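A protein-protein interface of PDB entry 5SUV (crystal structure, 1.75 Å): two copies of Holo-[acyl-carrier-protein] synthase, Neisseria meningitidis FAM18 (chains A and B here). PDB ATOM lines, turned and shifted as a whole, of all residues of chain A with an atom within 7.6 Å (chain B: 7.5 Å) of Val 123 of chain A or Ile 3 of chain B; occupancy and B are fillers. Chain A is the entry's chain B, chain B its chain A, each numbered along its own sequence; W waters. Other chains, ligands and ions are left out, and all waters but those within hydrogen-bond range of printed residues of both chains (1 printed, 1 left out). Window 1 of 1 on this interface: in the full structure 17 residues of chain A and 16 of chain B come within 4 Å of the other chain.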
ATOM      1  N   MET A   2      16.740   1.574 -26.463  1.00  0.00           N
ATOM      2  CA  MET A   2      15.346   1.867 -26.145  1.00  0.00           C
ATOM      3  C   MET A   2      15.234   2.660 -24.848  1.00  0.00           C
ATOM      4  O   MET A   2      14.623   3.731 -24.808  1.00  0.00           O
ATOM      5  CB  MET A   2      14.547   0.563 -26.027  1.00  0.00           C
ATOM      6  CG  MET A   2      13.088   0.739 -25.583  1.00  0.00           C
ATOM      7  SD  MET A   2      12.311  -0.802 -25.046  1.00  0.00           S
ATOM      8  CE  MET A   2      10.620  -0.274 -24.860  1.00  0.00           C
ATOM      9  N   ILE A   3      15.787   2.134 -23.778  1.00  0.00           N
ATOM     10  CA  ILE A   3      15.661   2.769 -22.478  1.00  0.00           C
ATOM     11  C   ILE A   3      16.866   3.671 -22.265  1.00  0.00           C
ATOM     12  O   ILE A   3      18.010   3.244 -22.433  1.00  0.00           O
ATOM     13  CB  ILE A   3      15.533   1.717 -21.366  1.00  0.00           C
ATOM     14  CG1 ILE A   3      14.179   1.014 -21.516  1.00  0.00           C
ATOM     15  CG2 ILE A   3      15.695   2.378 -19.997  1.00  0.00           C
ATOM     16  CD1 ILE A   3      13.905  -0.030 -20.488  1.00  0.00           C
ATOM     17  N   TYR A   4      16.599   4.927 -21.912  1.00  0.00           N
ATOM     18  CA  TYR A   4      17.667   5.855 -21.567  1.00  0.00           C
ATOM     19  C   TYR A   4      18.156   5.603 -20.150  1.00  0.00           C
ATOM     20  O   TYR A   4      19.368   5.574 -19.897  1.00  0.00           O
ATOM     21  CB  TYR A   4      17.177   7.290 -21.710  1.00  0.00           C
ATOM     22  CG  TYR A   4      18.263   8.299 -21.466  1.00  0.00           C
ATOM     23  CD1 TYR A   4      18.540   8.761 -20.186  1.00  0.00           C
ATOM     24  CD2 TYR A   4      19.018   8.792 -22.519  1.00  0.00           C
ATOM     25  CE1 TYR A   4      19.559   9.681 -19.962  1.00  0.00           C
ATOM     26  CE2 TYR A   4      20.019   9.713 -22.312  1.00  0.00           C
ATOM     27  CZ  TYR A   4      20.288  10.155 -21.035  1.00  0.00           C
ATOM     28  OH  TYR A   4      21.294  11.076 -20.865  1.00  0.00           O
ATOM     29  N   GLY A   5      17.230   5.390 -19.234  1.00  0.00           N
ATOM     30  CA  GLY A   5      17.585   5.089 -17.858  1.00  0.00           C
ATOM     31  C   GLY A   5      16.340   4.761 -17.067  1.00  0.00           C
ATOM     32  O   GLY A   5      15.218   5.006 -17.511  1.00  0.00           O
ATOM     33  N   ILE A   6      16.554   4.162 -15.900  1.00  0.00           N
ATOM     34  CA  ILE A   6      15.448   3.831 -15.020  1.00  0.00           C
ATOM     35  C   ILE A   6      15.754   4.400 -13.657  1.00  0.00           C
ATOM     36  O   ILE A   6      16.921   4.618 -13.304  1.00  0.00           O
ATOM     37  CB  ILE A   6      15.202   2.314 -14.925  1.00  0.00           C
ATOM     38  CG1 ILE A   6      16.421   1.588 -14.366  1.00  0.00           C
ATOM     39  CG2 ILE A   6      14.879   1.766 -16.296  1.00  0.00           C
ATOM     40  CD1 ILE A   6      16.225   0.077 -14.180  1.00  0.00           C
ATOM     41  N   GLY A   7      14.695   4.629 -12.894  1.00  0.00           N
ATOM     42  CA  GLY A   7      14.808   5.232 -11.583  1.00  0.00           C
ATOM     43  C   GLY A   7      13.739   4.701 -10.661  1.00  0.00           C
ATOM     44  O   GLY A   7      12.609   4.402 -11.064  1.00  0.00           O
ATOM     45  N   THR A   8      14.122   4.498  -9.406  1.00  0.00           N
ATOM     46  CA  THR A   8      13.164   4.143  -8.382  1.00  0.00           C
ATOM     47  C   THR A   8      13.532   4.942  -7.136  1.00  0.00           C
ATOM     48  O   THR A   8      14.681   5.356  -6.965  1.00  0.00           O
ATOM     49  CB  THR A   8      13.181   2.653  -8.089  1.00  0.00           C
ATOM     50  OG1 THR A   8      12.061   2.311  -7.264  1.00  0.00           O
ATOM     51  CG2 THR A   8      14.482   2.274  -7.390  1.00  0.00           C
ATOM     52  N   ALA A  59      13.207   9.770  -8.317  1.00  0.00           N
ATOM     53  CA  ALA A  59      13.246   8.666  -9.272  1.00  0.00           C
ATOM     54  C   ALA A  59      13.487   9.205 -10.678  1.00  0.00           C
ATOM     55  O   ALA A  59      14.259   8.629 -11.455  1.00  0.00           O
ATOM     56  CB  ALA A  59      11.957   7.838  -9.178  1.00  0.00           C
ATOM     57  N   PHE A  60      12.857  10.321 -11.003  1.00  0.00           N
ATOM     58  CA  PHE A  60      13.109  10.976 -12.277  1.00  0.00           C
ATOM     59  C   PHE A  60      14.580  11.307 -12.419  1.00  0.00           C
ATOM     60  O   PHE A  60      15.200  11.025 -13.450  1.00  0.00           O
ATOM     61  CB  PHE A  60      12.254  12.229 -12.382  1.00  0.00           C
ATOM     62  CG  PHE A  60      12.482  13.003 -13.646  1.00  0.00           C
ATOM     63  CD1 PHE A  60      13.536  13.904 -13.768  1.00  0.00           C
ATOM     64  CD2 PHE A  60      11.627  12.841 -14.701  1.00  0.00           C
ATOM     65  CE1 PHE A  60      13.727  14.607 -14.938  1.00  0.00           C
ATOM     66  CE2 PHE A  60      11.815  13.536 -15.872  1.00  0.00           C
ATOM     67  CZ  PHE A  60      12.868  14.422 -15.995  1.00  0.00           C
ATOM     68  N   ALA A  63      16.524   8.254 -13.211  1.00  0.00           N
ATOM     69  CA  ALA A  63      16.255   7.733 -14.546  1.00  0.00           C
ATOM     70  C   ALA A  63      16.965   8.539 -15.628  1.00  0.00           C
ATOM     71  O   ALA A  63      17.306   7.973 -16.676  1.00  0.00           O
ATOM     72  CB  ALA A  63      14.746   7.727 -14.824  1.00  0.00           C
ATOM     73  N   VAL A  64      17.152   9.854 -15.434  1.00  0.00           N
ATOM     74  CA  VAL A  64      17.832  10.650 -16.450  1.00  0.00           C
ATOM     75  C   VAL A  64      19.325  10.719 -16.193  1.00  0.00           C
ATOM     76  O   VAL A  64      20.043  11.372 -16.950  1.00  0.00           O
ATOM     77  CB  VAL A  64      17.218  12.059 -16.591  1.00  0.00           C
ATOM     78  CG1 VAL A  64      15.765  11.931 -17.025  1.00  0.00           C
ATOM     79  CG2 VAL A  64      17.347  12.898 -15.316  1.00  0.00           C
ATOM     80  N   PHE A  89       4.616  13.416 -16.095  1.00  0.00           N
ATOM     81  CA  PHE A  89       5.522  14.518 -15.801  1.00  0.00           C
ATOM     82  C   PHE A  89       5.249  15.719 -16.701  1.00  0.00           C
ATOM     83  O   PHE A  89       4.950  15.572 -17.890  1.00  0.00           O
ATOM     84  CB  PHE A  89       6.973  14.077 -15.997  1.00  0.00           C
ATOM     85  CG  PHE A  89       7.504  13.185 -14.937  1.00  0.00           C
ATOM     86  CD1 PHE A  89       7.684  13.644 -13.632  1.00  0.00           C
ATOM     87  CD2 PHE A  89       7.910  11.903 -15.252  1.00  0.00           C
ATOM     88  CE1 PHE A  89       8.193  12.819 -12.664  1.00  0.00           C
ATOM     89  CE2 PHE A  89       8.430  11.079 -14.305  1.00  0.00           C
ATOM     90  CZ  PHE A  89       8.589  11.536 -12.979  1.00  0.00           C
ATOM     91  N   ILE A 104      16.255  12.458 -24.732  1.00  0.00           N
ATOM     92  CA  ILE A 104      15.234  11.766 -23.956  1.00  0.00           C
ATOM     93  C   ILE A 104      13.874  12.150 -24.522  1.00  0.00           C
ATOM     94  O   ILE A 104      13.484  13.320 -24.476  1.00  0.00           O
ATOM     95  CB  ILE A 104      15.347  12.124 -22.470  1.00  0.00           C
ATOM     96  CG1 ILE A 104      16.719  11.700 -21.937  1.00  0.00           C
ATOM     97  CG2 ILE A 104      14.218  11.471 -21.663  1.00  0.00           C
ATOM     98  CD1 ILE A 104      17.061  12.315 -20.601  1.00  0.00           C
ATOM     99  N   ARG A 106      10.669  10.562 -23.839  1.00  0.00           N
ATOM    100  CA  ARG A 106       9.564  10.602 -22.909  1.00  0.00           C
ATOM    101  C   ARG A 106       9.927   9.826 -21.658  1.00  0.00           C
ATOM    102  O   ARG A 106      10.733   8.893 -21.694  1.00  0.00           O
ATOM    103  CB  ARG A 106       8.296  10.031 -23.525  1.00  0.00           C
ATOM    104  CG  ARG A 106       8.352   8.574 -23.751  1.00  0.00           C
ATOM    105  CD  ARG A 106       7.239   8.171 -24.672  1.00  0.00           C
ATOM    106  NE  ARG A 106       7.425   8.646 -26.036  1.00  0.00           N
ATOM    107  CZ  ARG A 106       8.093   7.980 -26.974  1.00  0.00           C
ATOM    108  NH1 ARG A 106       8.657   6.806 -26.706  1.00  0.00           N
ATOM    109  NH2 ARG A 106       8.203   8.494 -28.189  1.00  0.00           N
ATOM    110  N   VAL A 107       9.315  10.236 -20.560  1.00  0.00           N
ATOM    111  CA  VAL A 107       9.616   9.688 -19.245  1.00  0.00           C
ATOM    112  C   VAL A 107       8.303   9.305 -18.592  1.00  0.00           C
ATOM    113  O   VAL A 107       7.437  10.165 -18.406  1.00  0.00           O
ATOM    114  CB  VAL A 107      10.374  10.708 -18.392  1.00  0.00           C
ATOM    115  CG1 VAL A 107      10.799  10.096 -17.074  1.00  0.00           C
ATOM    116  CG2 VAL A 107      11.556  11.243 -19.167  1.00  0.00           C
ATOM    117  N   SER A 108       8.162   8.032 -18.239  1.00  0.00           N
ATOM    118  CA  SER A 108       6.953   7.500 -17.619  1.00  0.00           C
ATOM    119  C   SER A 108       7.121   7.375 -16.114  1.00  0.00           C
ATOM    120  O   SER A 108       8.232   7.241 -15.613  1.00  0.00           O
ATOM    121  CB  SER A 108       6.616   6.119 -18.166  1.00  0.00           C
ATOM    122  OG  SER A 108       6.352   6.123 -19.567  1.00  0.00           O
ATOM    123  N   LEU A 109       5.986   7.327 -15.409  1.00  0.00           N
ATOM    124  CA  LEU A 109       5.963   7.362 -13.958  1.00  0.00           C
ATOM    125  C   LEU A 109       4.867   6.468 -13.424  1.00  0.00           C
ATOM    126  O   LEU A 109       3.756   6.473 -13.955  1.00  0.00           O
ATOM    127  CB  LEU A 109       5.704   8.789 -13.472  1.00  0.00           C
ATOM    128  CG  LEU A 109       5.402   9.033 -12.003  1.00  0.00           C
ATOM    129  CD1 LEU A 109       6.565   8.667 -11.176  1.00  0.00           C
ATOM    130  CD2 LEU A 109       5.065  10.518 -11.805  1.00  0.00           C
ATOM    131  N   SER A 110       5.166   5.750 -12.354  1.00  0.00           N
ATOM    132  CA  SER A 110       4.123   5.113 -11.555  1.00  0.00           C
ATOM    133  C   SER A 110       4.456   5.312 -10.089  1.00  0.00           C
ATOM    134  O   SER A 110       5.629   5.410  -9.715  1.00  0.00           O
ATOM    135  CB  SER A 110       3.973   3.610 -11.852  1.00  0.00           C
ATOM    136  OG  SER A 110       2.876   3.044 -11.116  1.00  0.00           O
ATOM    137  N   PHE A 121       8.477   4.832  -9.467  1.00  0.00           N
ATOM    138  CA  PHE A 121       9.070   4.009 -10.516  1.00  0.00           C
ATOM    139  C   PHE A 121       9.063   4.870 -11.769  1.00  0.00           C
ATOM    140  O   PHE A 121       7.998   5.369 -12.157  1.00  0.00           O
ATOM    141  CB  PHE A 121       8.223   2.738 -10.701  1.00  0.00           C
ATOM    142  CG  PHE A 121       8.606   1.891 -11.885  1.00  0.00           C
ATOM    143  CD1 PHE A 121       9.891   1.907 -12.376  1.00  0.00           C
ATOM    144  CD2 PHE A 121       7.668   1.060 -12.497  1.00  0.00           C
ATOM    145  CE1 PHE A 121      10.245   1.121 -13.451  1.00  0.00           C
ATOM    146  CE2 PHE A 121       8.022   0.266 -13.560  1.00  0.00           C
ATOM    147  CZ  PHE A 121       9.313   0.303 -14.045  1.00  0.00           C
ATOM    148  N   VAL A 122      10.240   5.089 -12.383  1.00  0.00           N
ATOM    149  CA  VAL A 122      10.369   5.953 -13.552  1.00  0.00           C
ATOM    150  C   VAL A 122      11.178   5.238 -14.631  1.00  0.00           C
ATOM    151  O   VAL A 122      12.215   4.634 -14.351  1.00  0.00           O
ATOM    152  CB  VAL A 122      11.022   7.314 -13.201  1.00  0.00           C
ATOM    153  CG1 VAL A 122      11.292   8.144 -14.456  1.00  0.00           C
ATOM    154  CG2 VAL A 122      10.135   8.091 -12.246  1.00  0.00           C
ATOM    155  N   VAL A 123      10.722   5.354 -15.884  1.00  0.00           N
ATOM    156  CA  VAL A 123      11.480   4.866 -17.027  1.00  0.00           C
ATOM    157  C   VAL A 123      11.569   5.994 -18.043  1.00  0.00           C
ATOM    158  O   VAL A 123      10.542   6.526 -18.484  1.00  0.00           O
ATOM    159  CB  VAL A 123      10.860   3.614 -17.680  1.00  0.00           C
ATOM    160  CG1 VAL A 123      11.635   3.238 -18.932  1.00  0.00           C
ATOM    161  CG2 VAL A 123      10.868   2.457 -16.713  1.00  0.00           C
ATOM    162  N   ALA A 124      12.789   6.364 -18.384  1.00  0.00           N
ATOM    163  CA  ALA A 124      13.081   7.363 -19.403  1.00  0.00           C
ATOM    164  C   ALA A 124      13.458   6.648 -20.689  1.00  0.00           C
ATOM    165  O   ALA A 124      14.300   5.752 -20.675  1.00  0.00           O
ATOM    166  CB  ALA A 124      14.230   8.270 -18.945  1.00  0.00           C
ATOM    167  N   GLU A 125      12.823   7.030 -21.795  1.00  0.00           N
ATOM    168  CA  GLU A 125      13.084   6.413 -23.089  1.00  0.00           C
ATOM    169  C   GLU A 125      13.873   7.359 -23.979  1.00  0.00           C
ATOM    170  O   GLU A 125      13.738   8.576 -23.871  1.00  0.00           O
ATOM    171  CB  GLU A 125      11.775   6.063 -23.798  1.00  0.00           C
ATOM    172  CG  GLU A 125      11.007   4.980 -23.122  1.00  0.00           C
ATOM    173  CD  GLU A 125       9.644   4.809 -23.740  1.00  0.00           C
ATOM    174  OE1 GLU A 125       9.530   4.036 -24.714  1.00  0.00           O
ATOM    175  OE2 GLU A 125       8.709   5.493 -23.267  1.00  0.00           O
ATOM    176  N   LYS A 126      14.648   6.784 -24.903  1.00  0.00           N
ATOM    177  CA  LYS A 126      15.367   7.568 -25.911  1.00  0.00           C
ATOM    178  C   LYS A 126      14.470   7.912 -27.092  1.00  0.00           C
ATOM    179  O   LYS A 126      13.291   7.530 -27.125  1.00  0.00           O
ATOM    180  CB  LYS A 126      16.591   6.813 -26.414  1.00  0.00           C
ATOM    181  CG  LYS A 126      17.599   6.462 -25.344  1.00  0.00           C
ATOM    182  CD  LYS A 126      18.858   5.843 -25.957  1.00  0.00           C
ATOM    183  CE  LYS A 126      19.799   5.295 -24.899  1.00  0.00           C
ATOM    184  NZ  LYS A 126      20.885   4.480 -25.498  1.00  0.00           N
ATOM    185  N   ALA B   1       9.547  -0.358 -31.253  1.00  0.00           N
ATOM    186  CA  ALA B   1       8.796  -0.718 -30.015  1.00  0.00           C
ATOM    187  C   ALA B   1       8.996   0.356 -28.949  1.00  0.00           C
ATOM    188  O   ALA B   1      10.032   1.015 -28.912  1.00  0.00           O
ATOM    189  CB  ALA B   1       9.244  -2.083 -29.497  1.00  0.00           C
ATOM    190  N   MET B   2       8.001   0.531 -28.082  1.00  0.00           N
ATOM    191  CA  MET B   2       8.047   1.570 -27.067  1.00  0.00           C
ATOM    192  C   MET B   2       7.281   1.107 -25.838  1.00  0.00           C
ATOM    193  O   MET B   2       6.611   0.074 -25.843  1.00  0.00           O
ATOM    194  CB  MET B   2       7.439   2.876 -27.574  1.00  0.00           C
ATOM    195  CG  MET B   2       8.059   3.429 -28.840  1.00  0.00           C
ATOM    196  SD  MET B   2       7.214   4.923 -29.398  1.00  0.00           S
ATOM    197  CE  MET B   2       5.495   4.390 -29.435  1.00  0.00           C
ATOM    198  N   ILE B   3       7.347   1.904 -24.795  1.00  0.00           N
ATOM    199  CA  ILE B   3       6.619   1.593 -23.579  1.00  0.00           C
ATOM    200  C   ILE B   3       5.215   2.167 -23.687  1.00  0.00           C
ATOM    201  O   ILE B   3       5.038   3.337 -24.049  1.00  0.00           O
ATOM    202  CB  ILE B   3       7.371   2.123 -22.350  1.00  0.00           C
ATOM    203  CG1 ILE B   3       8.575   1.208 -22.127  1.00  0.00           C
ATOM    204  CG2 ILE B   3       6.491   2.128 -21.130  1.00  0.00           C
ATOM    205  CD1 ILE B   3       9.501   1.684 -21.087  1.00  0.00           C
ATOM    206  N   TYR B   4       4.210   1.320 -23.417  1.00  0.00           N
ATOM    207  CA  TYR B   4       2.827   1.779 -23.289  1.00  0.00           C
ATOM    208  C   TYR B   4       2.573   2.402 -21.923  1.00  0.00           C
ATOM    209  O   TYR B   4       1.916   3.447 -21.815  1.00  0.00           O
ATOM    210  CB  TYR B   4       1.862   0.606 -23.512  1.00  0.00           C
ATOM    211  CG  TYR B   4       0.417   1.010 -23.590  1.00  0.00           C
ATOM    212  CD1 TYR B   4      -0.333   1.216 -22.454  1.00  0.00           C
ATOM    213  CD2 TYR B   4      -0.200   1.183 -24.824  1.00  0.00           C
ATOM    214  CE1 TYR B   4      -1.644   1.612 -22.529  1.00  0.00           C
ATOM    215  CE2 TYR B   4      -1.504   1.559 -24.910  1.00  0.00           C
ATOM    216  CZ  TYR B   4      -2.224   1.770 -23.777  1.00  0.00           C
ATOM    217  OH  TYR B   4      -3.532   2.149 -23.888  1.00  0.00           O
ATOM    218  N   GLY B   5       3.086   1.776 -20.878  1.00  0.00           N
ATOM    219  CA  GLY B   5       2.988   2.324 -19.537  1.00  0.00           C
ATOM    220  C   GLY B   5       3.760   1.446 -18.582  1.00  0.00           C
ATOM    221  O   GLY B   5       4.182   0.344 -18.925  1.00  0.00           O
ATOM    222  N   ILE B   6       3.940   1.967 -17.371  1.00  0.00           N
ATOM    223  CA  ILE B   6       4.618   1.254 -16.302  1.00  0.00           C
ATOM    224  C   ILE B   6       3.747   1.341 -15.066  1.00  0.00           C
ATOM    225  O   ILE B   6       2.900   2.237 -14.932  1.00  0.00           O
ATOM    226  CB  ILE B   6       6.019   1.834 -16.021  1.00  0.00           C
ATOM    227  CG1 ILE B   6       5.901   3.271 -15.563  1.00  0.00           C
ATOM    228  CG2 ILE B   6       6.875   1.764 -17.275  1.00  0.00           C
ATOM    229  CD1 ILE B   6       7.287   3.890 -15.214  1.00  0.00           C
ATOM    230  N   ALA B  63      -0.034   0.041 -15.243  1.00  0.00           N
ATOM    231  CA  ALA B  63       0.836   0.008 -16.409  1.00  0.00           C
ATOM    232  C   ALA B  63       0.064   0.163 -17.712  1.00  0.00           C
ATOM    233  O   ALA B  63       0.643   0.575 -18.718  1.00  0.00           O
ATOM    234  CB  ALA B  63       1.621  -1.306 -16.431  1.00  0.00           C
ATOM    235  N   PHE B 121       6.364  -4.729  -9.887  1.00  0.00           N
ATOM    236  CA  PHE B 121       6.690  -3.817 -10.977  1.00  0.00           C
ATOM    237  C   PHE B 121       6.194  -4.428 -12.285  1.00  0.00           C
ATOM    238  O   PHE B 121       6.355  -5.629 -12.508  1.00  0.00           O
ATOM    239  CB  PHE B 121       8.193  -3.570 -11.107  1.00  0.00           C
ATOM    240  CG  PHE B 121       8.754  -2.592 -10.122  1.00  0.00           C
ATOM    241  CD1 PHE B 121       8.956  -2.949  -8.801  1.00  0.00           C
ATOM    242  CD2 PHE B 121       9.126  -1.323 -10.534  1.00  0.00           C
ATOM    243  CE1 PHE B 121       9.495  -2.047  -7.901  1.00  0.00           C
ATOM    244  CE2 PHE B 121       9.668  -0.415  -9.639  1.00  0.00           C
ATOM    245  CZ  PHE B 121       9.855  -0.779  -8.316  1.00  0.00           C
ATOM    246  N   VAL B 122       5.621  -3.596 -13.149  1.00  0.00           N
ATOM    247  CA  VAL B 122       5.063  -4.044 -14.417  1.00  0.00           C
ATOM    248  C   VAL B 122       5.432  -3.038 -15.497  1.00  0.00           C
ATOM    249  O   VAL B 122       5.293  -1.821 -15.303  1.00  0.00           O
ATOM    250  CB  VAL B 122       3.526  -4.193 -14.345  1.00  0.00           C
ATOM    251  CG1 VAL B 122       2.948  -4.500 -15.714  1.00  0.00           C
ATOM    252  CG2 VAL B 122       3.126  -5.272 -13.354  1.00  0.00           C
ATOM    253  N   VAL B 123       5.814  -3.553 -16.662  1.00  0.00           N
ATOM    254  CA  VAL B 123       6.017  -2.731 -17.847  1.00  0.00           C
ATOM    255  C   VAL B 123       5.193  -3.292 -18.990  1.00  0.00           C
ATOM    256  O   VAL B 123       5.372  -4.451 -19.379  1.00  0.00           O
ATOM    257  CB  VAL B 123       7.494  -2.665 -18.251  1.00  0.00           C
ATOM    258  CG1 VAL B 123       7.662  -1.775 -19.470  1.00  0.00           C
ATOM    259  CG2 VAL B 123       8.337  -2.166 -17.084  1.00  0.00           C
ATOM    260  N   ALA B 124       4.348  -2.456 -19.570  1.00  0.00           N
ATOM    261  CA  ALA B 124       3.584  -2.801 -20.757  1.00  0.00           C
ATOM    262  C   ALA B 124       4.242  -2.169 -21.978  1.00  0.00           C
ATOM    263  O   ALA B 124       4.538  -0.965 -21.977  1.00  0.00           O
ATOM    264  CB  ALA B 124       2.148  -2.321 -20.596  1.00  0.00           C
ATOM    265  N   GLU B 125       4.487  -2.975 -23.006  1.00  0.00           N
ATOM    266  CA  GLU B 125       5.169  -2.533 -24.216  1.00  0.00           C
ATOM    267  C   GLU B 125       4.220  -2.448 -25.400  1.00  0.00           C
ATOM    268  O   GLU B 125       3.281  -3.239 -25.520  1.00  0.00           O
ATOM    269  CB  GLU B 125       6.295  -3.479 -24.620  1.00  0.00           C
ATOM    270  CG  GLU B 125       7.405  -3.618 -23.642  1.00  0.00           C
ATOM    271  CD  GLU B 125       8.318  -4.731 -24.058  1.00  0.00           C
ATOM    272  OE1 GLU B 125       9.059  -4.535 -25.038  1.00  0.00           O
ATOM    273  OE2 GLU B 125       8.248  -5.813 -23.451  1.00  0.00           O
ATOM    274  N   LYS B 126       4.536  -1.498 -26.279  1.00  0.00           N
ATOM    275  CA  LYS B 126       3.870  -1.211 -27.554  1.00  0.00           C
ATOM    276  C   LYS B 126       2.478  -0.637 -27.369  1.00  0.00           C
ATOM    277  O   LYS B 126       2.271   0.556 -27.587  1.00  0.00           O
ATOM    278  CB  LYS B 126       3.806  -2.454 -28.432  1.00  0.00           C
ATOM    279  CG  LYS B 126       5.147  -2.915 -28.939  1.00  0.00           C
ATOM    280  CD  LYS B 126       4.961  -4.059 -29.914  1.00  0.00           C
ATOM    281  CE  LYS B 126       6.037  -4.121 -30.978  1.00  0.00           C
ATOM    282  NZ  LYS B 126       5.748  -5.238 -31.923  1.00  0.00           N
HETATM  283  O   HOH W   1       1.677   4.793 -14.546  1.00  0.00           O
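The backbone carbonyl oxygen (O) of Met 2 of chain B is in hydrogen-bond range of the backbone NH (N) of Lys 126 of chain B, at 2.6 Å.
The backbone carbonyl oxygen of Met 2 of chain A lies within hydrogen-bond range of the backbone NH of Lys 126 of chain A.
The guanidinium group of Arg 106 of chain A is in salt-bridge range of the side-chain carboxylate of Glu 125 of chain A (3.5 Å).
The backbone NH (N) of Ser 108 of chain A sits at hydrogen-bond distance from the backbone carbonyl oxygen (O) of Val 123 of chain A (2.8 Å).
N of Ser 110 of chain A sits at hydrogen-bond distance from O of Phe 121 of chain A (2.9 Å).
Among the printed residues, pairs that only touch across the chains: Phe 121 of chain A with Phe 121 of chain B (3.4 Å), Val 123 of chain A with Ile 3 of chain B (3.4 Å), Phe 121 of chain A with Ile 6 of chain B (3.5 Å), Ser 108 of chain A with Ile 6 of chain B (3.5 Å), Ser 110 of chain A with Ile 6 of chain B (3.5 Å), Leu 109 of chain A with Ile 6 of chain B (3.7 Å), Glu 125 of chain A with Met 2 of chain B (3.7 Å), Met 2 of chain A with Ile 3 of chain B (3.7 Å), Met 2 of chain A with Met 2 of chain B (3.7 Å), Val 123 of chain A with Ile 6 of chain B (3.8 Å), Phe 121 of chain A with Val 122 of chain B (3.9 Å) and Thr 8 of chain A with Phe 121 of chain B (3.9 Å).
Met 2 of chain A touches Ile 3 of chain B, but with the chains exchanged Ile 3 of chain A does not touch Met 2 of chain B (8.1 Å).
Phe 121 of chain B touches its own counterpart, Phe 121 of chain A.
Val 123 of chain A touches Ile 3 of chain B, but with the chains exchanged Ile 3 of chain A does not touch Val 123 of chain B (6.6 Å).
Glu 125 of chain A touches Ile 3 of chain B, but with the chains exchanged Ile 3 of chain A does not touch Glu 125 of chain B (8.0 Å).
Of the 14 pairs that touch across the chains among the printed residues, 2 have their exchanged pair printed and touching as well.
Hydrophobic or aromatic side chains of chain A that line the printed part of chain B: Met 2, Phe 121 and Val 123.
Of the 13 printed residues of chain B, 5 touch a printed residue of chain A.
Hydrophobic or aromatic side chains of chain B within 4 Å of the printed part of chain A: Met 2, Ile 3, Ile 6 and Phe 121.
Among the printed residues, 14 pairs touch across the chains.
Among the printed residues, no Asp or Glu carboxylate lies within 4 Å of a Lys or Arg side-chain nitrogen of the other chain.
SD of Met 2 of chain B is in hydrogen-bond range of NH1 of Arg 106 of chain A (3.6 Å).
The backbone NH of Ile 3 of chain B sits at hydrogen-bond distance from the side-chain carboxylate of Glu 125 of chain A (3.1 Å).
Water W1 bridges O of Leu 109 of chain A (2.7 Å) and O of Ile 6 of chain B (2.9 Å).
Ile 3 of chain A touches none of the printed residues of chain B.
Phe 89 of chain A touches none of the printed residues of chain B.
Printed residues of chain B within 4 Å of Arg 106 of chain A: Met 2 (3.6 Å).
Of chain B, only Ile 3 and Ile 6 come within 4 Å of Val 123 of chain A.
Ile 3 of chain B touches just these residues of chain A: Met 2, Val 123 and Glu 125.
Printed residues of chain A within 4 Å of Val 122 of chain B: Phe 121 (3.9 Å).
The nearest residue of chain B that does not touch Val 123 of chain A is Val 123 of chain B (5.3 Å).
The nearest residue of chain A that does not touch Ile 3 of chain B is Ser 108 of chain A (4.3 Å).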
